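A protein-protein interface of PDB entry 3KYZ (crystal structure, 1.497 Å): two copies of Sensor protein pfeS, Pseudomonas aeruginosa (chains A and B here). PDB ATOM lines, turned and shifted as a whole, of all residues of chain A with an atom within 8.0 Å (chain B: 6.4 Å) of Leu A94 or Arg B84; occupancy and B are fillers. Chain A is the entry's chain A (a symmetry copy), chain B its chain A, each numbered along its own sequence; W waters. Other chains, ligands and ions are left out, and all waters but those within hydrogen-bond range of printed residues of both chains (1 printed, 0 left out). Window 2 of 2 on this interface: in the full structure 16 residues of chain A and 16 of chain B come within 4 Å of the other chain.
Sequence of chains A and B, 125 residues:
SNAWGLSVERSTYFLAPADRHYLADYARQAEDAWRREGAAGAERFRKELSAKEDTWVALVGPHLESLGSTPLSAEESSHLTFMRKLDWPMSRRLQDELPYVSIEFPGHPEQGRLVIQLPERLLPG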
ATOM      1  N   TYR A  13     -12.871  18.006   0.763  1.00  0.00           N
ATOM      2  CA  TYR A  13     -14.035  17.152   0.549  1.00  0.00           C
ATOM      3  C   TYR A  13     -13.752  15.686   0.881  1.00  0.00           C
ATOM      4  O   TYR A  13     -14.656  14.857   0.859  1.00  0.00           O
ATOM      5  CB  TYR A  13     -14.544  17.289  -0.889  1.00  0.00           C
ATOM      6  CG  TYR A  13     -15.848  18.048  -0.996  1.00  0.00           C
ATOM      7  CD1 TYR A  13     -16.881  17.587  -1.804  1.00  0.00           C
ATOM      8  CD2 TYR A  13     -16.053  19.217  -0.275  1.00  0.00           C
ATOM      9  CE1 TYR A  13     -18.078  18.279  -1.900  1.00  0.00           C
ATOM     10  CE2 TYR A  13     -17.247  19.913  -0.363  1.00  0.00           C
ATOM     11  CZ  TYR A  13     -18.255  19.441  -1.175  1.00  0.00           C
ATOM     12  OH  TYR A  13     -19.440  20.135  -1.260  1.00  0.00           O
ATOM     13  N   THR A  81     -28.794   2.931   1.773  1.00  0.00           N
ATOM     14  CA  THR A  81     -28.919   2.905   0.315  1.00  0.00           C
ATOM     15  C   THR A  81     -28.085   3.933  -0.445  1.00  0.00           C
ATOM     16  O   THR A  81     -27.877   3.776  -1.654  1.00  0.00           O
ATOM     17  CB  THR A  81     -30.396   3.068  -0.123  1.00  0.00           C
ATOM     18  OG1 THR A  81     -30.926   4.277   0.437  1.00  0.00           O
ATOM     19  CG2 THR A  81     -31.230   1.886   0.343  1.00  0.00           C
ATOM     20  N   PHE A  82     -27.613   4.975   0.246  1.00  0.00           N
ATOM     21  CA  PHE A  82     -26.887   6.071  -0.404  1.00  0.00           C
ATOM     22  C   PHE A  82     -25.609   6.371   0.367  1.00  0.00           C
ATOM     23  O   PHE A  82     -25.281   7.532   0.654  1.00  0.00           O
ATOM     24  CB  PHE A  82     -27.757   7.334  -0.508  1.00  0.00           C
ATOM     25  CG  PHE A  82     -29.100   7.100  -1.139  1.00  0.00           C
ATOM     26  CD1 PHE A  82     -29.200   6.642  -2.449  1.00  0.00           C
ATOM     27  CD2 PHE A  82     -30.266   7.363  -0.432  1.00  0.00           C
ATOM     28  CE1 PHE A  82     -30.449   6.425  -3.031  1.00  0.00           C
ATOM     29  CE2 PHE A  82     -31.514   7.158  -1.010  1.00  0.00           C
ATOM     30  CZ  PHE A  82     -31.605   6.682  -2.311  1.00  0.00           C
ATOM     31  N   MET A  83     -24.887   5.304   0.699  1.00  0.00           N
ATOM     32  CA  MET A  83     -23.727   5.398   1.570  1.00  0.00           C
ATOM     33  C   MET A  83     -22.464   5.819   0.839  1.00  0.00           C
ATOM     34  O   MET A  83     -22.436   5.865  -0.397  1.00  0.00           O
ATOM     35  CB  MET A  83     -23.518   4.071   2.300  1.00  0.00           C
ATOM     36  CG  MET A  83     -24.737   3.673   3.130  1.00  0.00           C
ATOM     37  SD  MET A  83     -24.352   2.326   4.465  1.00  0.00           S
ATOM     38  CE  MET A  83     -24.308   0.758   3.336  1.00  0.00           C
ATOM     39  N   ARG A  84     -21.428   6.141   1.615  1.00  0.00           N
ATOM     40  CA  ARG A  84     -20.123   6.516   1.074  1.00  0.00           C
ATOM     41  C   ARG A  84     -19.041   5.625   1.666  1.00  0.00           C
ATOM     42  O   ARG A  84     -19.119   5.249   2.841  1.00  0.00           O
ATOM     43  CB  ARG A  84     -19.786   7.974   1.419  1.00  0.00           C
ATOM     44  CG  ARG A  84     -20.909   8.970   1.170  1.00  0.00           C
ATOM     45  CD  ARG A  84     -21.235   9.092  -0.309  1.00  0.00           C
ATOM     46  NE  ARG A  84     -20.172   9.781  -1.033  1.00  0.00           N
ATOM     47  CZ  ARG A  84     -20.064   9.813  -2.357  1.00  0.00           C
ATOM     48  NH1 ARG A  84     -20.958   9.187  -3.117  1.00  0.00           N
ATOM     49  NH2 ARG A  84     -19.058  10.470  -2.922  1.00  0.00           N
ATOM     50  N   TRP A  88     -14.113   8.150  -0.426  1.00  0.00           N
ATOM     51  CA  TRP A  88     -14.947   8.878  -1.369  1.00  0.00           C
ATOM     52  C   TRP A  88     -15.160  10.310  -0.894  1.00  0.00           C
ATOM     53  O   TRP A  88     -15.051  10.594   0.294  1.00  0.00           O
ATOM     54  CB  TRP A  88     -16.309   8.190  -1.512  1.00  0.00           C
ATOM     55  CG  TRP A  88     -16.265   6.840  -2.157  1.00  0.00           C
ATOM     56  CD1 TRP A  88     -15.153   6.138  -2.553  1.00  0.00           C
ATOM     57  CD2 TRP A  88     -17.395   6.024  -2.489  1.00  0.00           C
ATOM     58  NE1 TRP A  88     -15.532   4.933  -3.110  1.00  0.00           N
ATOM     59  CE2 TRP A  88     -16.901   4.839  -3.074  1.00  0.00           C
ATOM     60  CE3 TRP A  88     -18.776   6.181  -2.341  1.00  0.00           C
ATOM     61  CZ2 TRP A  88     -17.742   3.821  -3.519  1.00  0.00           C
ATOM     62  CZ3 TRP A  88     -19.611   5.165  -2.777  1.00  0.00           C
ATOM     63  CH2 TRP A  88     -19.089   4.001  -3.364  1.00  0.00           C
ATOM     64  N   SER A  91     -19.912  14.980   1.806  1.00  0.00           N
ATOM     65  CA  SER A  91     -20.609  16.256   1.950  1.00  0.00           C
ATOM     66  C   SER A  91     -22.047  16.089   2.434  1.00  0.00           C
ATOM     67  O   SER A  91     -22.632  15.011   2.316  1.00  0.00           O
ATOM     68  CB  SER A  91     -20.597  17.029   0.630  1.00  0.00           C
ATOM     69  OG  SER A  91     -21.780  16.788  -0.107  1.00  0.00           O
ATOM     70  N   ARG A  92     -22.600  17.170   2.984  1.00  0.00           N
ATOM     71  CA  ARG A  92     -23.989  17.176   3.427  1.00  0.00           C
ATOM     72  C   ARG A  92     -24.916  17.557   2.276  1.00  0.00           C
ATOM     73  O   ARG A  92     -26.121  17.316   2.337  1.00  0.00           O
ATOM     74  CB  ARG A  92     -24.180  18.159   4.587  1.00  0.00           C
ATOM     75  CG  ARG A  92     -23.204  17.981   5.740  1.00  0.00           C
ATOM     76  CD  ARG A  92     -23.423  19.035   6.818  1.00  0.00           C
ATOM     77  NE  ARG A  92     -24.607  18.758   7.628  1.00  0.00           N
ATOM     78  CZ  ARG A  92     -24.592  18.616   8.950  1.00  0.00           C
ATOM     79  NH1 ARG A  92     -25.719  18.362   9.605  1.00  0.00           N
ATOM     80  NH2 ARG A  92     -23.454  18.734   9.620  1.00  0.00           N
ATOM     81  N   ARG A  93     -24.339  18.151   1.234  1.00  0.00           N
ATOM     82  CA  ARG A  93     -25.079  18.665   0.078  1.00  0.00           C
ATOM     83  C   ARG A  93     -26.297  17.844  -0.349  1.00  0.00           C
ATOM     84  O   ARG A  93     -27.441  18.224  -0.086  1.00  0.00           O
ATOM     85  CB  ARG A  93     -24.138  18.820  -1.123  1.00  0.00           C
ATOM     86  CG  ARG A  93     -23.144  19.969  -1.013  1.00  0.00           C
ATOM     87  CD  ARG A  93     -23.743  21.277  -1.511  1.00  0.00           C
ATOM     88  NE  ARG A  93     -22.752  22.349  -1.562  1.00  0.00           N
ATOM     89  CZ  ARG A  93     -22.063  22.683  -2.652  1.00  0.00           C
ATOM     90  NH1 ARG A  93     -22.258  22.031  -3.791  1.00  0.00           N
ATOM     91  NH2 ARG A  93     -21.182  23.674  -2.601  1.00  0.00           N
ATOM     92  N   LEU A  94     -26.032  16.724  -1.016  1.00  0.00           N
ATOM     93  CA  LEU A  94     -27.061  15.965  -1.727  1.00  0.00           C
ATOM     94  C   LEU A  94     -28.300  15.612  -0.901  1.00  0.00           C
ATOM     95  O   LEU A  94     -29.413  15.605  -1.428  1.00  0.00           O
ATOM     96  CB  LEU A  94     -26.450  14.697  -2.339  1.00  0.00           C
ATOM     97  CG  LEU A  94     -26.621  14.492  -3.846  1.00  0.00           C
ATOM     98  CD1 LEU A  94     -26.318  15.768  -4.621  1.00  0.00           C
ATOM     99  CD2 LEU A  94     -25.741  13.348  -4.326  1.00  0.00           C
ATOM    100  N   GLN A  95     -28.116  15.322   0.384  1.00  0.00           N
ATOM    101  CA  GLN A  95     -29.234  14.872   1.214  1.00  0.00           C
ATOM    102  C   GLN A  95     -29.469  15.674   2.495  1.00  0.00           C
ATOM    103  O   GLN A  95     -30.325  15.319   3.306  1.00  0.00           O
ATOM    104  CB  GLN A  95     -29.082  13.393   1.553  1.00  0.00           C
ATOM    105  CG  GLN A  95     -29.292  12.481   0.363  1.00  0.00           C
ATOM    106  CD  GLN A  95     -29.734  11.101   0.777  1.00  0.00           C
ATOM    107  OE1 GLN A  95     -28.919  10.274   1.182  1.00  0.00           O
ATOM    108  NE2 GLN A  95     -31.035  10.842   0.682  1.00  0.00           N
ATOM    109  N   ASP A  96     -28.711  16.749   2.675  1.00  0.00           N
ATOM    110  CA  ASP A  96     -28.892  17.628   3.827  1.00  0.00           C
ATOM    111  C   ASP A  96     -28.818  16.870   5.154  1.00  0.00           C
ATOM    112  O   ASP A  96     -29.638  17.070   6.050  1.00  0.00           O
ATOM    113  CB  ASP A  96     -30.223  18.375   3.725  1.00  0.00           C
ATOM    114  CG  ASP A  96     -30.306  19.542   4.684  1.00  0.00           C
ATOM    115  OD1 ASP A  96     -29.241  20.005   5.145  1.00  0.00           O
ATOM    116  OD2 ASP A  96     -31.434  19.997   4.972  1.00  0.00           O
ATOM    117  N   GLU A  97     -27.827  15.996   5.268  1.00  0.00           N
ATOM    118  CA  GLU A  97     -27.570  15.264   6.502  1.00  0.00           C
ATOM    119  C   GLU A  97     -26.155  14.729   6.414  1.00  0.00           C
ATOM    120  O   GLU A  97     -25.584  14.644   5.324  1.00  0.00           O
ATOM    121  CB  GLU A  97     -28.550  14.101   6.665  1.00  0.00           C
ATOM    122  CG  GLU A  97     -28.430  13.053   5.565  1.00  0.00           C
ATOM    123  CD  GLU A  97     -29.408  11.900   5.720  1.00  0.00           C
ATOM    124  OE1 GLU A  97     -29.382  10.985   4.867  1.00  0.00           O
ATOM    125  OE2 GLU A  97     -30.199  11.903   6.688  1.00  0.00           O
ATOM    126  N   PHE B  82     -25.021   1.918  -2.633  1.00  0.00           N
ATOM    127  CA  PHE B  82     -24.350   3.112  -3.158  1.00  0.00           C
ATOM    128  C   PHE B  82     -25.119   3.650  -4.357  1.00  0.00           C
ATOM    129  O   PHE B  82     -24.541   3.974  -5.406  1.00  0.00           O
ATOM    130  CB  PHE B  82     -22.894   2.811  -3.547  1.00  0.00           C
ATOM    131  CG  PHE B  82     -22.096   2.152  -2.458  1.00  0.00           C
ATOM    132  CD1 PHE B  82     -21.882   2.797  -1.244  1.00  0.00           C
ATOM    133  CD2 PHE B  82     -21.535   0.898  -2.656  1.00  0.00           C
ATOM    134  CE1 PHE B  82     -21.141   2.182  -0.235  1.00  0.00           C
ATOM    135  CE2 PHE B  82     -20.786   0.284  -1.658  1.00  0.00           C
ATOM    136  CZ  PHE B  82     -20.594   0.925  -0.443  1.00  0.00           C
ATOM    137  N   MET B  83     -26.435   3.742  -4.190  1.00  0.00           N
ATOM    138  CA  MET B  83     -27.330   4.082  -5.283  1.00  0.00           C
ATOM    139  C   MET B  83     -27.425   5.577  -5.535  1.00  0.00           C
ATOM    140  O   MET B  83     -26.933   6.383  -4.735  1.00  0.00           O
ATOM    141  CB  MET B  83     -28.714   3.483  -5.026  1.00  0.00           C
ATOM    142  CG  MET B  83     -28.664   1.965  -4.874  1.00  0.00           C
ATOM    143  SD  MET B  83     -30.389   1.113  -5.081  1.00  0.00           S
ATOM    144  CE  MET B  83     -31.151   1.504  -3.349  1.00  0.00           C
ATOM    145  N   ARG B  84     -28.046   5.935  -6.659  1.00  0.00           N
ATOM    146  CA  ARG B  84     -28.271   7.332  -7.027  1.00  0.00           C
ATOM    147  C   ARG B  84     -29.752   7.568  -7.284  1.00  0.00           C
ATOM    148  O   ARG B  84     -30.439   6.689  -7.815  1.00  0.00           O
ATOM    149  CB  ARG B  84     -27.498   7.692  -8.304  1.00  0.00           C
ATOM    150  CG  ARG B  84     -26.049   7.233  -8.330  1.00  0.00           C
ATOM    151  CD  ARG B  84     -25.214   7.945  -7.279  1.00  0.00           C
ATOM    152  NE  ARG B  84     -25.002   9.346  -7.626  1.00  0.00           N
ATOM    153  CZ  ARG B  84     -24.531  10.265  -6.790  1.00  0.00           C
ATOM    154  NH1 ARG B  84     -24.219   9.934  -5.539  1.00  0.00           N
ATOM    155  NH2 ARG B  84     -24.373  11.516  -7.203  1.00  0.00           N
ATOM    156  N   LYS B  85     -30.246   8.749  -6.922  1.00  0.00           N
ATOM    157  CA  LYS B  85     -31.600   9.145  -7.304  1.00  0.00           C
ATOM    158  C   LYS B  85     -31.599   9.779  -8.689  1.00  0.00           C
ATOM    159  O   LYS B  85     -30.554  10.205  -9.187  1.00  0.00           O
ATOM    160  CB  LYS B  85     -32.210  10.097  -6.277  1.00  0.00           C
ATOM    161  CG  LYS B  85     -32.497   9.436  -4.932  1.00  0.00           C
ATOM    162  CD  LYS B  85     -33.307  10.364  -4.049  1.00  0.00           C
ATOM    163  CE  LYS B  85     -33.511   9.773  -2.662  1.00  0.00           C
ATOM    164  NZ  LYS B  85     -34.322  10.670  -1.795  1.00  0.00           N
ATOM    165  N   LEU B  86     -32.775   9.846  -9.307  1.00  0.00           N
ATOM    166  CA  LEU B  86     -32.883  10.268 -10.704  1.00  0.00           C
ATOM    167  C   LEU B  86     -32.305  11.652 -10.992  1.00  0.00           C
ATOM    168  O   LEU B  86     -31.847  11.909 -12.110  1.00  0.00           O
ATOM    169  CB  LEU B  86     -34.335  10.214 -11.174  1.00  0.00           C
ATOM    170  CG  LEU B  86     -34.877   8.809 -11.455  1.00  0.00           C
ATOM    171  CD1 LEU B  86     -36.389   8.835 -11.639  1.00  0.00           C
ATOM    172  CD2 LEU B  86     -34.196   8.208 -12.676  1.00  0.00           C
ATOM    173  N   ASP B  87     -32.344  12.550 -10.011  1.00  0.00           N
ATOM    174  CA  ASP B  87     -31.860  13.913 -10.243  1.00  0.00           C
ATOM    175  C   ASP B  87     -30.462  14.185  -9.699  1.00  0.00           C
ATOM    176  O   ASP B  87     -30.028  15.339  -9.620  1.00  0.00           O
ATOM    177  CB  ASP B  87     -32.857  14.955  -9.736  1.00  0.00           C
ATOM    178  CG  ASP B  87     -33.133  14.836  -8.258  1.00  0.00           C
ATOM    179  OD1 ASP B  87     -32.815  13.785  -7.657  1.00  0.00           O
ATOM    180  OD2 ASP B  87     -33.687  15.808  -7.698  1.00  0.00           O
ATOM    181  N   TRP B  88     -29.754  13.121  -9.333  1.00  0.00           N
ATOM    182  CA  TRP B  88     -28.395  13.254  -8.830  1.00  0.00           C
ATOM    183  C   TRP B  88     -27.392  13.116  -9.969  1.00  0.00           C
ATOM    184  O   TRP B  88     -27.694  12.516 -10.996  1.00  0.00           O
ATOM    185  CB  TRP B  88     -28.112  12.173  -7.782  1.00  0.00           C
ATOM    186  CG  TRP B  88     -28.896  12.308  -6.514  1.00  0.00           C
ATOM    187  CD1 TRP B  88     -29.875  13.230  -6.230  1.00  0.00           C
ATOM    188  CD2 TRP B  88     -28.762  11.492  -5.345  1.00  0.00           C
ATOM    189  NE1 TRP B  88     -30.354  13.027  -4.951  1.00  0.00           N
ATOM    190  CE2 TRP B  88     -29.691  11.963  -4.393  1.00  0.00           C
ATOM    191  CE3 TRP B  88     -27.949  10.404  -5.015  1.00  0.00           C
ATOM    192  CZ2 TRP B  88     -29.822  11.387  -3.131  1.00  0.00           C
ATOM    193  CZ3 TRP B  88     -28.085   9.827  -3.762  1.00  0.00           C
ATOM    194  CH2 TRP B  88     -29.013  10.324  -2.834  1.00  0.00           C
ATOM    195  N   PRO B  89     -26.178  13.653  -9.784  1.00  0.00           N
ATOM    196  CA  PRO B  89     -25.139  13.444 -10.800  1.00  0.00           C
ATOM    197  C   PRO B  89     -24.892  11.952 -11.038  1.00  0.00           C
ATOM    198  O   PRO B  89     -24.943  11.168 -10.088  1.00  0.00           O
ATOM    199  CB  PRO B  89     -23.897  14.095 -10.178  1.00  0.00           C
ATOM    200  CG  PRO B  89     -24.427  15.043  -9.151  1.00  0.00           C
ATOM    201  CD  PRO B  89     -25.691  14.427  -8.631  1.00  0.00           C
ATOM    202  N   MET B  90     -24.632  11.577 -12.288  1.00  0.00           N
ATOM    203  CA  MET B  90     -24.418  10.181 -12.676  1.00  0.00           C
ATOM    204  C   MET B  90     -23.045   9.987 -13.303  1.00  0.00           C
ATOM    205  O   MET B  90     -22.632  10.776 -14.153  1.00  0.00           O
ATOM    206  CB  MET B  90     -25.457   9.760 -13.714  1.00  0.00           C
ATOM    207  CG  MET B  90     -26.887   9.920 -13.279  1.00  0.00           C
ATOM    208  SD  MET B  90     -27.582   8.290 -12.506  1.00  0.00           S
ATOM    209  CE  MET B  90     -29.197   9.050 -11.722  1.00  0.00           C
ATOM    210  N   SER B  91     -22.351   8.922 -12.913  1.00  0.00           N
ATOM    211  CA  SER B  91     -21.074   8.596 -13.544  1.00  0.00           C
ATOM    212  C   SER B  91     -20.600   7.182 -13.218  1.00  0.00           C
ATOM    213  O   SER B  91     -21.041   6.579 -12.238  1.00  0.00           O
ATOM    214  CB  SER B  91     -19.999   9.606 -13.138  1.00  0.00           C
ATOM    215  OG  SER B  91     -19.252   9.132 -12.034  1.00  0.00           O
ATOM    216  N   PRO B  99     -24.282   3.159 -12.739  1.00  0.00           N
ATOM    217  CA  PRO B  99     -24.910   3.395 -11.431  1.00  0.00           C
ATOM    218  C   PRO B  99     -26.192   2.588 -11.229  1.00  0.00           C
ATOM    219  O   PRO B  99     -26.922   2.321 -12.190  1.00  0.00           O
ATOM    220  CB  PRO B  99     -25.278   4.883 -11.471  1.00  0.00           C
ATOM    221  CG  PRO B  99     -24.517   5.463 -12.600  1.00  0.00           C
ATOM    222  CD  PRO B  99     -24.229   4.371 -13.572  1.00  0.00           C
ATOM    223  N   TYR B 100     -26.461   2.215  -9.982  1.00  0.00           N
ATOM    224  CA  TYR B 100     -27.762   1.651  -9.632  1.00  0.00           C
ATOM    225  C   TYR B 100     -28.672   2.790  -9.214  1.00  0.00           C
ATOM    226  O   TYR B 100     -28.346   3.550  -8.301  1.00  0.00           O
ATOM    227  CB  TYR B 100     -27.635   0.606  -8.520  1.00  0.00           C
ATOM    228  CG  TYR B 100     -26.862  -0.601  -8.981  1.00  0.00           C
ATOM    229  CD1 TYR B 100     -27.494  -1.629  -9.671  1.00  0.00           C
ATOM    230  CD2 TYR B 100     -25.498  -0.706  -8.743  1.00  0.00           C
ATOM    231  CE1 TYR B 100     -26.789  -2.729 -10.114  1.00  0.00           C
ATOM    232  CE2 TYR B 100     -24.787  -1.792  -9.177  1.00  0.00           C
ATOM    233  CZ  TYR B 100     -25.435  -2.805  -9.864  1.00  0.00           C
ATOM    234  OH  TYR B 100     -24.724  -3.890 -10.286  1.00  0.00           O
ATOM    235  N   VAL B 101     -29.797   2.919  -9.909  1.00  0.00           N
ATOM    236  CA  VAL B 101     -30.715   4.022  -9.684  1.00  0.00           C
ATOM    237  C   VAL B 101     -31.887   3.572  -8.818  1.00  0.00           C
ATOM    238  O   VAL B 101     -32.529   2.557  -9.103  1.00  0.00           O
ATOM    239  CB  VAL B 101     -31.234   4.582 -11.024  1.00  0.00           C
ATOM    240  CG1 VAL B 101     -32.166   5.764 -10.788  1.00  0.00           C
ATOM    241  CG2 VAL B 101     -30.060   4.976 -11.918  1.00  0.00           C
ATOM    242  N   SER B 102     -32.137   4.328  -7.750  1.00  0.00           N
ATOM    243  CA  SER B 102     -33.199   4.049  -6.791  1.00  0.00           C
ATOM    244  C   SER B 102     -34.377   4.976  -7.060  1.00  0.00           C
ATOM    245  O   SER B 102     -34.220   6.200  -7.074  1.00  0.00           O
ATOM    246  CB  SER B 102     -32.680   4.313  -5.379  1.00  0.00           C
ATOM    247  OG  SER B 102     -33.685   4.133  -4.399  1.00  0.00           O
ATOM    248  N   ILE B 103     -35.553   4.399  -7.278  1.00  0.00           N
ATOM    249  CA  ILE B 103     -36.747   5.186  -7.594  1.00  0.00           C
ATOM    250  C   ILE B 103     -37.924   4.720  -6.738  1.00  0.00           C
ATOM    251  O   ILE B 103     -38.453   3.619  -6.923  1.00  0.00           O
ATOM    252  CB  ILE B 103     -37.135   5.086  -9.087  1.00  0.00           C
ATOM    253  CG1 ILE B 103     -35.912   5.253 -10.000  1.00  0.00           C
ATOM    254  CG2 ILE B 103     -38.231   6.110  -9.416  1.00  0.00           C
ATOM    255  CD1 ILE B 103     -36.153   4.807 -11.456  1.00  0.00           C
HETATM  256  O   HOH W   1     -32.329  14.199  -2.555  1.00  0.00           O
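O of Thr A81 is in hydrogen-bond range of N of Met B83, 2.9 Å away.
The guanidinium group of Arg B84 lies within hydrogen-bond range of the backbone carbonyl oxygen of Pro B89, at 3.0 Å. The backbone carbonyl oxygen (O) of Tyr B100 sits at hydrogen-bond distance from the backbone NH (N) of Arg B84, at 2.9 Å. The backbone carbonyl oxygen of Arg B84 sits at hydrogen-bond distance from the backbone NH of Ser B102, at 2.9 Å.
Among the printed residues, pairs that only touch across the chains: Phe A82 with Met B83 (3.2 Å), Met A83 with Phe B82 (3.2 Å), Thr A81 with Phe B82 (3.5 Å), Phe A82 with Trp B88 (3.6 Å), Trp A88 with Phe B82 (3.6 Å), Phe A82 with Lys B85 (3.6 Å), Leu A94 with Arg B84 (3.7 Å), Leu A94 with Trp B88 (3.7 Å), Gln A95 with Trp B88 (3.7 Å) and Phe A82 with Ser B102 (3.9 Å).
Of the printed residues of chain B, Phe A82 touches Met B83, Lys B85, Trp B88 and Ser B102. Printed residues of chain B within 4 Å of Met A83: Phe B82 (3.2 Å). Of chain B, only Arg B84 and Trp B88 come within 4 Å of Leu A94. Printed residues of chain B within 4 Å of Gln A95: Trp B88 (3.7 Å). Asp A96 touches none of the printed residues of chain B. Glu A97 touches none of the printed residues of chain B. Of the printed residues of chain A, Met B83 touches Thr A81 (2.9 Å) and Phe A82 (3.2 Å). Arg B84 touches one residue of chain A. Of the printed residues of chain A, Trp B88 touches Phe A82 (3.6 Å), Leu A94 (3.7 Å) and Gln A95 (3.7 Å). The nearest residue of chain A that does not touch Arg B84 is Arg A84 (4.1 Å). The nearest printed residue of chain A that does not touch Lys B85 is Gln A95 (4.1 Å).
Of the 15 printed residues of chain B, 6 touch a printed residue of chain A. Printed residues of chain B that touch a printed residue of chain A: Phe B82, Met B83, Arg B84, Lys B85, Trp B88 and Ser B102. Of the 13 printed residues of chain A, 6 touch a printed residue of chain B. Hydrophobic or aromatic side chains of chain A within 4 Å of the printed part of chain B: Phe A82, Met A83, Trp A88 and Leu A94. Among the printed residues, 11 pairs touch across the chains.
Phe A82 touches Met B83, and with the chains exchanged Met A83 touches Phe B82. Phe A82 touches Trp B88, and with the chains exchanged Trp A88 touches Phe B82. Of the 11 pairs that touch across the chains among the printed residues, 4 have their exchanged pair printed and touching as well.
Water W1 bridges NE1 of Trp B88 and O of Leu A94.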
